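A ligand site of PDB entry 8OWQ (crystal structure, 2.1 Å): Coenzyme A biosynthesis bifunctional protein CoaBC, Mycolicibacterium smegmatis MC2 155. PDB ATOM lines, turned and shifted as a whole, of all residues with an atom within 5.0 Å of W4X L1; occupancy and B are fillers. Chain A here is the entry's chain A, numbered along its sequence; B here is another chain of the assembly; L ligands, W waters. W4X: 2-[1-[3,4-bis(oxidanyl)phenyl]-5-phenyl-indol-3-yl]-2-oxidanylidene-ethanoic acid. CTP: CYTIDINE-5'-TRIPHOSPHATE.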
ATOM      1  N   GLY A  20     -12.381   3.162  24.767  1.00  0.00           N
ATOM      2  CA  GLY A  20     -11.555   2.706  25.863  1.00  0.00           C
ATOM      3  C   GLY A  20     -10.295   2.023  25.360  1.00  0.00           C
ATOM      4  O   GLY A  20      -9.942   2.085  24.186  1.00  0.00           O
ATOM      5  N   ASN A  34      -3.105   0.567  28.544  1.00  0.00           N
ATOM      6  CA  ASN A  34      -2.704   1.906  28.126  1.00  0.00           C
ATOM      7  C   ASN A  34      -3.586   2.957  28.823  1.00  0.00           C
ATOM      8  O   ASN A  34      -4.508   2.621  29.573  1.00  0.00           O
ATOM      9  CB  ASN A  34      -2.752   2.019  26.595  1.00  0.00           C
ATOM     10  CG  ASN A  34      -4.136   2.299  26.041  1.00  0.00           C
ATOM     11  OD1 ASN A  34      -5.159   1.977  26.646  1.00  0.00           O
ATOM     12  ND2 ASN A  34      -4.175   2.890  24.862  1.00  0.00           N
ATOM     13  N   SER A  36      -5.774   5.261  27.697  1.00  0.00           N
ATOM     14  CA  SER A  36      -6.958   5.780  27.011  1.00  0.00           C
ATOM     15  C   SER A  36      -8.124   5.985  27.960  1.00  0.00           C
ATOM     16  O   SER A  36      -8.496   5.082  28.711  1.00  0.00           O
ATOM     17  CB  SER A  36      -7.368   4.830  25.898  1.00  0.00           C
ATOM     18  OG  SER A  36      -6.466   4.916  24.843  1.00  0.00           O
ATOM     19  N   SER A  37      -8.737   7.174  27.902  1.00  0.00           N
ATOM     20  CA  SER A  37      -9.848   7.493  28.792  1.00  0.00           C
ATOM     21  C   SER A  37     -11.187   6.981  28.279  1.00  0.00           C
ATOM     22  O   SER A  37     -12.093   6.733  29.084  1.00  0.00           O
ATOM     23  CB  SER A  37      -9.946   9.005  28.985  1.00  0.00           C
ATOM     24  OG  SER A  37     -10.282   9.635  27.760  1.00  0.00           O
ATOM     25  N   GLY A  38     -11.380   6.860  26.975  1.00  0.00           N
ATOM     26  CA  GLY A  38     -12.688   6.562  26.438  1.00  0.00           C
ATOM     27  C   GLY A  38     -13.596   7.754  26.240  1.00  0.00           C
ATOM     28  O   GLY A  38     -14.653   7.606  25.612  1.00  0.00           O
ATOM     29  N   LYS A  39     -13.181   8.951  26.687  1.00  0.00           N
ATOM     30  CA  LYS A  39     -14.086  10.096  26.781  1.00  0.00           C
ATOM     31  C   LYS A  39     -14.573  10.562  25.411  1.00  0.00           C
ATOM     32  O   LYS A  39     -15.764  10.853  25.248  1.00  0.00           O
ATOM     33  CB  LYS A  39     -13.400  11.252  27.508  1.00  0.00           C
ATOM     34  CG  LYS A  39     -13.293  11.043  28.996  1.00  0.00           C
ATOM     35  CD  LYS A  39     -12.304  12.031  29.580  1.00  0.00           C
ATOM     36  CE  LYS A  39     -12.322  12.014  31.082  1.00  0.00           C
ATOM     37  NZ  LYS A  39     -11.617  13.202  31.633  1.00  0.00           N
ATOM     38  N   GLN A  40     -13.675  10.675  24.436  1.00  0.00           N
ATOM     39  CA  GLN A  40     -14.113  11.142  23.124  1.00  0.00           C
ATOM     40  C   GLN A  40     -15.022  10.136  22.430  1.00  0.00           C
ATOM     41  O   GLN A  40     -15.945  10.530  21.711  1.00  0.00           O
ATOM     42  CB  GLN A  40     -12.892  11.469  22.243  1.00  0.00           C
ATOM     43  CG  GLN A  40     -13.223  12.200  20.921  1.00  0.00           C
ATOM     44  CD  GLN A  40     -13.910  13.534  21.128  1.00  0.00           C
ATOM     45  OE1 GLN A  40     -13.255  14.581  21.266  1.00  0.00           O
ATOM     46  NE2 GLN A  40     -15.244  13.527  21.147  1.00  0.00           N
ATOM     47  N   GLY A  41     -14.774   8.839  22.633  1.00  0.00           N
ATOM     48  CA  GLY A  41     -15.645   7.820  22.073  1.00  0.00           C
ATOM     49  C   GLY A  41     -16.987   7.706  22.747  1.00  0.00           C
ATOM     50  O   GLY A  41     -17.975   7.377  22.082  1.00  0.00           O
ATOM     51  N   ALA A  99     -13.363   3.640  18.042  1.00  0.00           N
ATOM     52  CA  ALA A  99     -12.595   4.599  18.805  1.00  0.00           C
ATOM     53  C   ALA A  99     -11.674   3.942  19.824  1.00  0.00           C
ATOM     54  O   ALA A  99     -10.780   4.624  20.341  1.00  0.00           O
ATOM     55  CB  ALA A  99     -13.513   5.601  19.502  1.00  0.00           C
ATOM     56  N   ALA A 100     -11.833   2.650  20.096  1.00  0.00           N
ATOM     57  CA  ALA A 100     -11.049   1.985  21.136  1.00  0.00           C
ATOM     58  C   ALA A 100      -9.568   1.943  20.760  1.00  0.00           C
ATOM     59  O   ALA A 100      -9.208   1.900  19.584  1.00  0.00           O
ATOM     60  CB  ALA A 100     -11.565   0.560  21.346  1.00  0.00           C
ATOM     61  N   ALA A 101      -8.712   1.936  21.787  1.00  0.00           N
ATOM     62  CA  ALA A 101      -7.307   1.571  21.604  1.00  0.00           C
ATOM     63  C   ALA A 101      -7.220   0.067  21.788  1.00  0.00           C
ATOM     64  O   ALA A 101      -7.296  -0.422  22.908  1.00  0.00           O
ATOM     65  CB  ALA A 101      -6.409   2.310  22.589  1.00  0.00           C
ATOM     66  N   PHE A 155     -10.227   5.702  14.235  1.00  0.00           N
ATOM     67  CA  PHE A 155      -9.669   6.755  15.059  1.00  0.00           C
ATOM     68  C   PHE A 155      -8.155   6.615  15.087  1.00  0.00           C
ATOM     69  O   PHE A 155      -7.630   5.512  14.910  1.00  0.00           O
ATOM     70  CB  PHE A 155     -10.213   6.684  16.502  1.00  0.00           C
ATOM     71  CG  PHE A 155     -11.432   7.522  16.759  1.00  0.00           C
ATOM     72  CD1 PHE A 155     -11.429   8.487  17.755  1.00  0.00           C
ATOM     73  CD2 PHE A 155     -12.596   7.329  16.026  1.00  0.00           C
ATOM     74  CE1 PHE A 155     -12.565   9.257  18.016  1.00  0.00           C
ATOM     75  CE2 PHE A 155     -13.729   8.100  16.273  1.00  0.00           C
ATOM     76  CZ  PHE A 155     -13.714   9.058  17.271  1.00  0.00           C
ATOM     77  N   ALA A 156      -7.456   7.720  15.312  1.00  0.00           N
ATOM     78  CA  ALA A 156      -6.005   7.662  15.417  1.00  0.00           C
ATOM     79  C   ALA A 156      -5.537   8.828  16.274  1.00  0.00           C
ATOM     80  O   ALA A 156      -6.148   9.906  16.278  1.00  0.00           O
ATOM     81  CB  ALA A 156      -5.329   7.699  14.052  1.00  0.00           C
ATOM     82  N   ALA A 157      -4.438   8.598  17.019  1.00  0.00           N
ATOM     83  CA  ALA A 157      -3.756   9.625  17.792  1.00  0.00           C
ATOM     84  C   ALA A 157      -2.339   9.717  17.251  1.00  0.00           C
ATOM     85  O   ALA A 157      -1.516   8.826  17.502  1.00  0.00           O
ATOM     86  CB  ALA A 157      -3.758   9.293  19.279  1.00  0.00           C
ATOM     87  N   VAL A 183     -10.566   9.657  11.989  1.00  0.00           N
ATOM     88  CA  VAL A 183     -10.543  10.793  12.887  1.00  0.00           C
ATOM     89  C   VAL A 183      -9.177  10.793  13.568  1.00  0.00           C
ATOM     90  O   VAL A 183      -8.799   9.808  14.224  1.00  0.00           O
ATOM     91  CB  VAL A 183     -11.690  10.708  13.894  1.00  0.00           C
ATOM     92  CG1 VAL A 183     -11.790  11.999  14.712  1.00  0.00           C
ATOM     93  CG2 VAL A 183     -13.007  10.422  13.191  1.00  0.00           C
ATOM     94  N   VAL A 184      -8.441  11.878  13.405  1.00  0.00           N
ATOM     95  CA  VAL A 184      -7.062  11.964  13.875  1.00  0.00           C
ATOM     96  C   VAL A 184      -6.993  13.071  14.908  1.00  0.00           C
ATOM     97  O   VAL A 184      -7.311  14.233  14.612  1.00  0.00           O
ATOM     98  CB  VAL A 184      -6.073  12.242  12.726  1.00  0.00           C
ATOM     99  CG1 VAL A 184      -4.642  12.116  13.206  1.00  0.00           C
ATOM    100  CG2 VAL A 184      -6.300  11.301  11.564  1.00  0.00           C
ATOM    101  N   ASN A 185      -6.557  12.721  16.109  1.00  0.00           N
ATOM    102  CA  ASN A 185      -6.228  13.703  17.123  1.00  0.00           C
ATOM    103  C   ASN A 185      -4.732  13.948  17.059  1.00  0.00           C
ATOM    104  O   ASN A 185      -3.939  13.002  17.138  1.00  0.00           O
ATOM    105  CB  ASN A 185      -6.648  13.207  18.509  1.00  0.00           C
ATOM    106  CG  ASN A 185      -6.238  14.157  19.622  1.00  0.00           C
ATOM    107  OD1 ASN A 185      -6.147  15.375  19.422  1.00  0.00           O
ATOM    108  ND2 ASN A 185      -5.991  13.603  20.800  1.00  0.00           N
ATOM    109  N   LEU A 212      -9.604  19.397  12.421  1.00  0.00           N
ATOM    110  CA  LEU A 212     -10.393  19.343  13.660  1.00  0.00           C
ATOM    111  C   LEU A 212      -9.948  20.468  14.576  1.00  0.00           C
ATOM    112  O   LEU A 212      -8.858  20.412  15.153  1.00  0.00           O
ATOM    113  CB  LEU A 212     -10.228  17.999  14.363  1.00  0.00           C
ATOM    114  CG  LEU A 212     -11.270  16.919  14.126  1.00  0.00           C
ATOM    115  CD1 LEU A 212     -11.209  15.952  15.297  1.00  0.00           C
ATOM    116  CD2 LEU A 212     -12.634  17.526  14.001  1.00  0.00           C
ATOM    117  N   LYS A 217     -14.824  17.693  24.357  1.00  0.00           N
ATOM    118  CA  LYS A 217     -15.210  16.402  23.797  1.00  0.00           C
ATOM    119  C   LYS A 217     -16.553  16.484  23.101  1.00  0.00           C
ATOM    120  O   LYS A 217     -16.742  15.901  22.028  1.00  0.00           O
ATOM    121  CB  LYS A 217     -15.279  15.330  24.901  1.00  0.00           C
ATOM    122  CG  LYS A 217     -13.998  15.113  25.676  1.00  0.00           C
ATOM    123  CD  LYS A 217     -13.098  14.134  24.962  1.00  0.00           C
ATOM    124  CE  LYS A 217     -11.735  14.736  24.700  1.00  0.00           C
ATOM    125  NZ  LYS A 217     -11.137  14.162  23.462  1.00  0.00           N
ATOM    126  N   MET A 220     -16.245  18.517  19.706  1.00  0.00           N
ATOM    127  CA  MET A 220     -15.575  17.706  18.695  1.00  0.00           C
ATOM    128  C   MET A 220     -16.367  16.460  18.350  1.00  0.00           C
ATOM    129  O   MET A 220     -16.366  16.036  17.190  1.00  0.00           O
ATOM    130  CB  MET A 220     -14.166  17.344  19.157  1.00  0.00           C
ATOM    131  CG  MET A 220     -13.383  18.580  19.529  1.00  0.00           C
ATOM    132  SD  MET A 220     -11.613  18.336  19.473  1.00  0.00           S
ATOM    133  CE  MET A 220     -11.323  17.659  21.113  1.00  0.00           C
ATOM    134  N   ILE A 224     -17.321  15.357  14.592  1.00  0.00           N
ATOM    135  CA  ILE A 224     -17.140  14.011  14.066  1.00  0.00           C
ATOM    136  C   ILE A 224     -18.457  13.469  13.513  1.00  0.00           C
ATOM    137  O   ILE A 224     -18.509  12.931  12.399  1.00  0.00           O
ATOM    138  CB  ILE A 224     -16.557  13.082  15.151  1.00  0.00           C
ATOM    139  CG1 ILE A 224     -15.138  13.524  15.517  1.00  0.00           C
ATOM    140  CG2 ILE A 224     -16.586  11.612  14.701  1.00  0.00           C
ATOM    141  CD1 ILE A 224     -14.733  13.076  16.910  1.00  0.00           C
ATOM    142  N   ARG B  30       1.581   3.024  27.144  1.00  0.00           N
ATOM    143  CA  ARG B  30       1.254   1.693  27.646  1.00  0.00           C
ATOM    144  C   ARG B  30       2.096   1.341  28.855  1.00  0.00           C
ATOM    145  O   ARG B  30       3.059   2.040  29.197  1.00  0.00           O
ATOM    146  CB  ARG B  30       1.401   0.661  26.535  1.00  0.00           C
ATOM    147  CG  ARG B  30       0.507   0.969  25.352  1.00  0.00           C
ATOM    148  CD  ARG B  30       1.340   1.012  24.106  1.00  0.00           C
ATOM    149  NE  ARG B  30       0.564   1.314  22.921  1.00  0.00           N
ATOM    150  CZ  ARG B  30       1.088   1.393  21.697  1.00  0.00           C
ATOM    151  NH1 ARG B  30       0.322   1.674  20.649  1.00  0.00           N
ATOM    152  NH2 ARG B  30       2.398   1.201  21.539  1.00  0.00           N
ATOM    153  N   LYS B 114       5.734   6.232  21.271  1.00  0.00           N
ATOM    154  CA  LYS B 114       4.813   5.112  21.117  1.00  0.00           C
ATOM    155  C   LYS B 114       5.457   4.009  20.293  1.00  0.00           C
ATOM    156  O   LYS B 114       5.858   4.225  19.146  1.00  0.00           O
ATOM    157  CB  LYS B 114       3.522   5.607  20.448  1.00  0.00           C
ATOM    158  CG  LYS B 114       2.346   4.692  20.588  1.00  0.00           C
ATOM    159  CD  LYS B 114       1.096   5.478  20.357  1.00  0.00           C
ATOM    160  CE  LYS B 114       0.249   4.907  19.264  1.00  0.00           C
ATOM    161  NZ  LYS B 114      -0.952   5.765  19.072  1.00  0.00           N
HETATM  162  C10 W4X L   1      -7.962   7.800  20.457  1.00  0.00           C
HETATM  163  C13 W4X L   1      -8.925   7.500  22.456  1.00  0.00           C
HETATM  164  C17 W4X L   1      -6.895   4.773  19.337  1.00  0.00           C
HETATM  165  C20 W4X L   1      -4.316   4.984  20.372  1.00  0.00           C
HETATM  166  C21 W4X L   1      -5.337   5.782  20.839  1.00  0.00           C
HETATM  167  C24 W4X L   1      -9.770   7.653  23.749  1.00  0.00           C
HETATM  168  C01 W4X L   1     -10.141  13.901  20.068  1.00  0.00           C
HETATM  169  C02 W4X L   1     -10.524  14.156  18.752  1.00  0.00           C
HETATM  170  C03 W4X L   1     -10.425  13.166  17.793  1.00  0.00           C
HETATM  171  C04 W4X L   1      -9.971  11.913  18.152  1.00  0.00           C
HETATM  172  C05 W4X L   1      -9.610  11.647  19.464  1.00  0.00           C
HETATM  173  C06 W4X L   1      -9.671  12.650  20.430  1.00  0.00           C
HETATM  174  C07 W4X L   1      -9.070  10.277  19.841  1.00  0.00           C
HETATM  175  C08 W4X L   1      -8.187   9.680  18.957  1.00  0.00           C
HETATM  176  C09 W4X L   1      -7.637   8.439  19.260  1.00  0.00           C
HETATM  177  C11 W4X L   1      -8.823   8.395  21.352  1.00  0.00           C
HETATM  178  C12 W4X L   1      -9.380   9.652  21.048  1.00  0.00           C
HETATM  179  C14 W4X L   1      -8.118   6.424  22.125  1.00  0.00           C
HETATM  180  C16 W4X L   1      -6.616   5.692  20.341  1.00  0.00           C
HETATM  181  C18 W4X L   1      -5.877   3.954  18.862  1.00  0.00           C
HETATM  182  C19 W4X L   1      -4.593   4.073  19.382  1.00  0.00           C
HETATM  183  C25 W4X L   1     -11.013   8.512  23.737  1.00  0.00           C
HETATM  184  N15 W4X L   1      -7.567   6.609  20.945  1.00  0.00           N
HETATM  185  O22 W4X L   1      -3.020   5.096  20.894  1.00  0.00           O
HETATM  186  O23 W4X L   1      -3.555   3.264  18.925  1.00  0.00           O
HETATM  187  O26 W4X L   1     -10.945   9.709  24.113  1.00  0.00           O
HETATM  188  O27 W4X L   1     -12.088   7.981  23.353  1.00  0.00           O
HETATM  189  O28 W4X L   1      -9.507   7.119  24.772  1.00  0.00           O
HETATM  190  N1  CTP L   2      -7.682  -1.082  15.780  1.00  0.00           N
HETATM  191  C2  CTP L   2      -8.296  -2.304  15.587  1.00  0.00           C
HETATM  192  N3  CTP L   2      -7.617  -3.460  15.935  1.00  0.00           N
HETATM  193  C4  CTP L   2      -6.275  -3.419  16.270  1.00  0.00           C
HETATM  194  C5  CTP L   2      -5.612  -2.193  16.306  1.00  0.00           C
HETATM  195  C6  CTP L   2      -6.318  -1.036  15.975  1.00  0.00           C
HETATM  196  O2  CTP L   2      -9.431  -2.336  15.100  1.00  0.00           O
HETATM  197  N4  CTP L   2      -5.621  -4.532  16.565  1.00  0.00           N
HETATM  198  C1' CTP L   2      -8.395   0.116  15.320  1.00  0.00           C
HETATM  199  C2' CTP L   2      -8.499   1.187  16.396  1.00  0.00           C
HETATM  200  O2' CTP L   2      -9.688   1.127  17.175  1.00  0.00           O
HETATM  201  C3' CTP L   2      -8.397   2.477  15.612  1.00  0.00           C
HETATM  202  C4' CTP L   2      -7.658   2.094  14.345  1.00  0.00           C
HETATM  203  O4' CTP L   2      -7.643   0.682  14.262  1.00  0.00           O
HETATM  204  O3' CTP L   2      -9.675   2.954  15.232  1.00  0.00           O
HETATM  205  C5' CTP L   2      -6.238   2.630  14.284  1.00  0.00           C
HETATM  206  O5' CTP L   2      -5.562   2.488  15.529  1.00  0.00           O
HETATM  207  PA  CTP L   2      -3.941   2.571  15.502  1.00  0.00           P
HETATM  208  O1A CTP L   2      -3.343   1.947  16.742  1.00  0.00           O
HETATM  209  O2A CTP L   2      -3.419   3.964  15.234  1.00  0.00           O
HETATM  210  O3A CTP L   2      -3.652   1.627  14.252  1.00  0.00           O
HETATM  211  PB  CTP L   2      -2.218   0.944  14.121  1.00  0.00           P
HETATM  212  O1B CTP L   2      -2.294  -0.452  14.713  1.00  0.00           O
HETATM  213  O2B CTP L   2      -1.912   0.873  12.650  1.00  0.00           O
HETATM  214  O3B CTP L   2      -1.277   1.994  14.980  1.00  0.00           O
HETATM  215  PG  CTP L   2       0.330   2.318  14.907  1.00  0.00           P
HETATM  216  O1G CTP L   2       1.076   1.001  14.860  1.00  0.00           O
HETATM  217  O2G CTP L   2       0.676   3.173  13.706  1.00  0.00           O
HETATM  218  O3G CTP L   2       0.771   3.090  16.134  1.00  0.00           O
HETATM  219  O   HOH W   1      -2.119   3.091  22.809  1.00  0.00           O
HETATM  220  O   HOH W   2      -1.689   7.732  21.899  1.00  0.00           O
HETATM  221  O   HOH W   3     -12.001   5.589  23.030  1.00  0.00           O
HETATM  222  O   HOH W   4      -5.465   0.540  18.591  1.00  0.00           O
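Residues that only touch W4X L1: Ser 36 (3.3 Å), Ala 156 (3.4 Å), Asn 185 (3.5 Å), Lys 217 (3.5 Å), Val 183 (3.6 Å), Phe 155 (3.6 Å), Ala 99 (3.7 Å), Ala 100 (3.7 Å), Leu 212 (3.8 Å), Ala 101 (3.9 Å) and Ala 157 (3.9 Å).
Hydrophobic or aromatic side chains that line W4X L1: Phe 155, Ala 157, Val 183 and Leu 212.
The nearest printed residue that does not touch W4X L1 is Met 220 (4.1 Å).
Water W3 lies within hydrogen-bond range of an oxygen (O27) of W4X L1 (2.4 Å), the backbone NH of Gly 20 (3.0 Å) and the backbone carbonyl oxygen of Ala 99 (3.1 Å).
Water W1 lies within hydrogen-bond range of ND2 of Asn 34 (2.9 Å), O22 of W4X L1 (2.9 Å) and NE of Arg 30 of chain B (3.2 Å).
Water W4 lies within hydrogen-bond range of O1A of CTP L2 (3.1 Å) and O23 of W4X L1 (3.3 Å).
O23 of W4X L1 lies within hydrogen-bond range of O1A of CTP L2.
O2' of CTP L2 is in hydrogen-bond range of O of Ala 100.
The side-chain amino group (NZ) of Lys 114 of chain B is in hydrogen-bond range of an oxygen (O22) of W4X L1, at 2.8 Å.
N of Gly 41 lies within hydrogen-bond range of O27 of W4X L1, at 2.9 Å.
An oxygen (O28) of W4X L1 lies within hydrogen-bond range of the backbone NH (N) of Ser 37 (3.2 Å).
N of Gly 38 sits at hydrogen-bond distance from O28 of W4X L1, at 2.9 Å.
The backbone NH (N) of Gln 40 lies within hydrogen-bond range of an oxygen (O26) of W4X L1, 2.9 Å away.
The backbone NH (N) of Lys 39 sits at hydrogen-bond distance from an oxygen (O26) of W4X L1 (3.5 Å).
The backbone NH (N) of Phe 155 lies within hydrogen-bond range of an oxygen (O3') of CTP L2 (3.0 Å).
The backbone carbonyl oxygen (O) of Phe 155 sits close to an oxygen (O3') of CTP L2.
The backbone NH (N) of Ala 101 is in hydrogen-bond range of the backbone carbonyl oxygen (O) of Gly 20, at 2.7 Å.
The backbone carbonyl oxygen (O) of Lys 217 is in hydrogen-bond range of the side-chain amide nitrogen (NE2) of Gln 40, at 2.9 Å.
N of Asn 185 sits at hydrogen-bond distance from O of Ala 156.
The backbone NH of Lys 39 sits at hydrogen-bond distance from the side-chain hydroxyl of Ser 37 (3.2 Å).
The side-chain amide nitrogen (ND2) of Asn 34 sits at hydrogen-bond distance from the side-chain hydroxyl (OG) of Ser 36 (3.1 Å).
N of Ala 156 is in hydrogen-bond range of O of Val 183.
The side-chain amino group of Lys 114 of chain B sits at hydrogen-bond distance from the backbone carbonyl oxygen of Ala 157.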
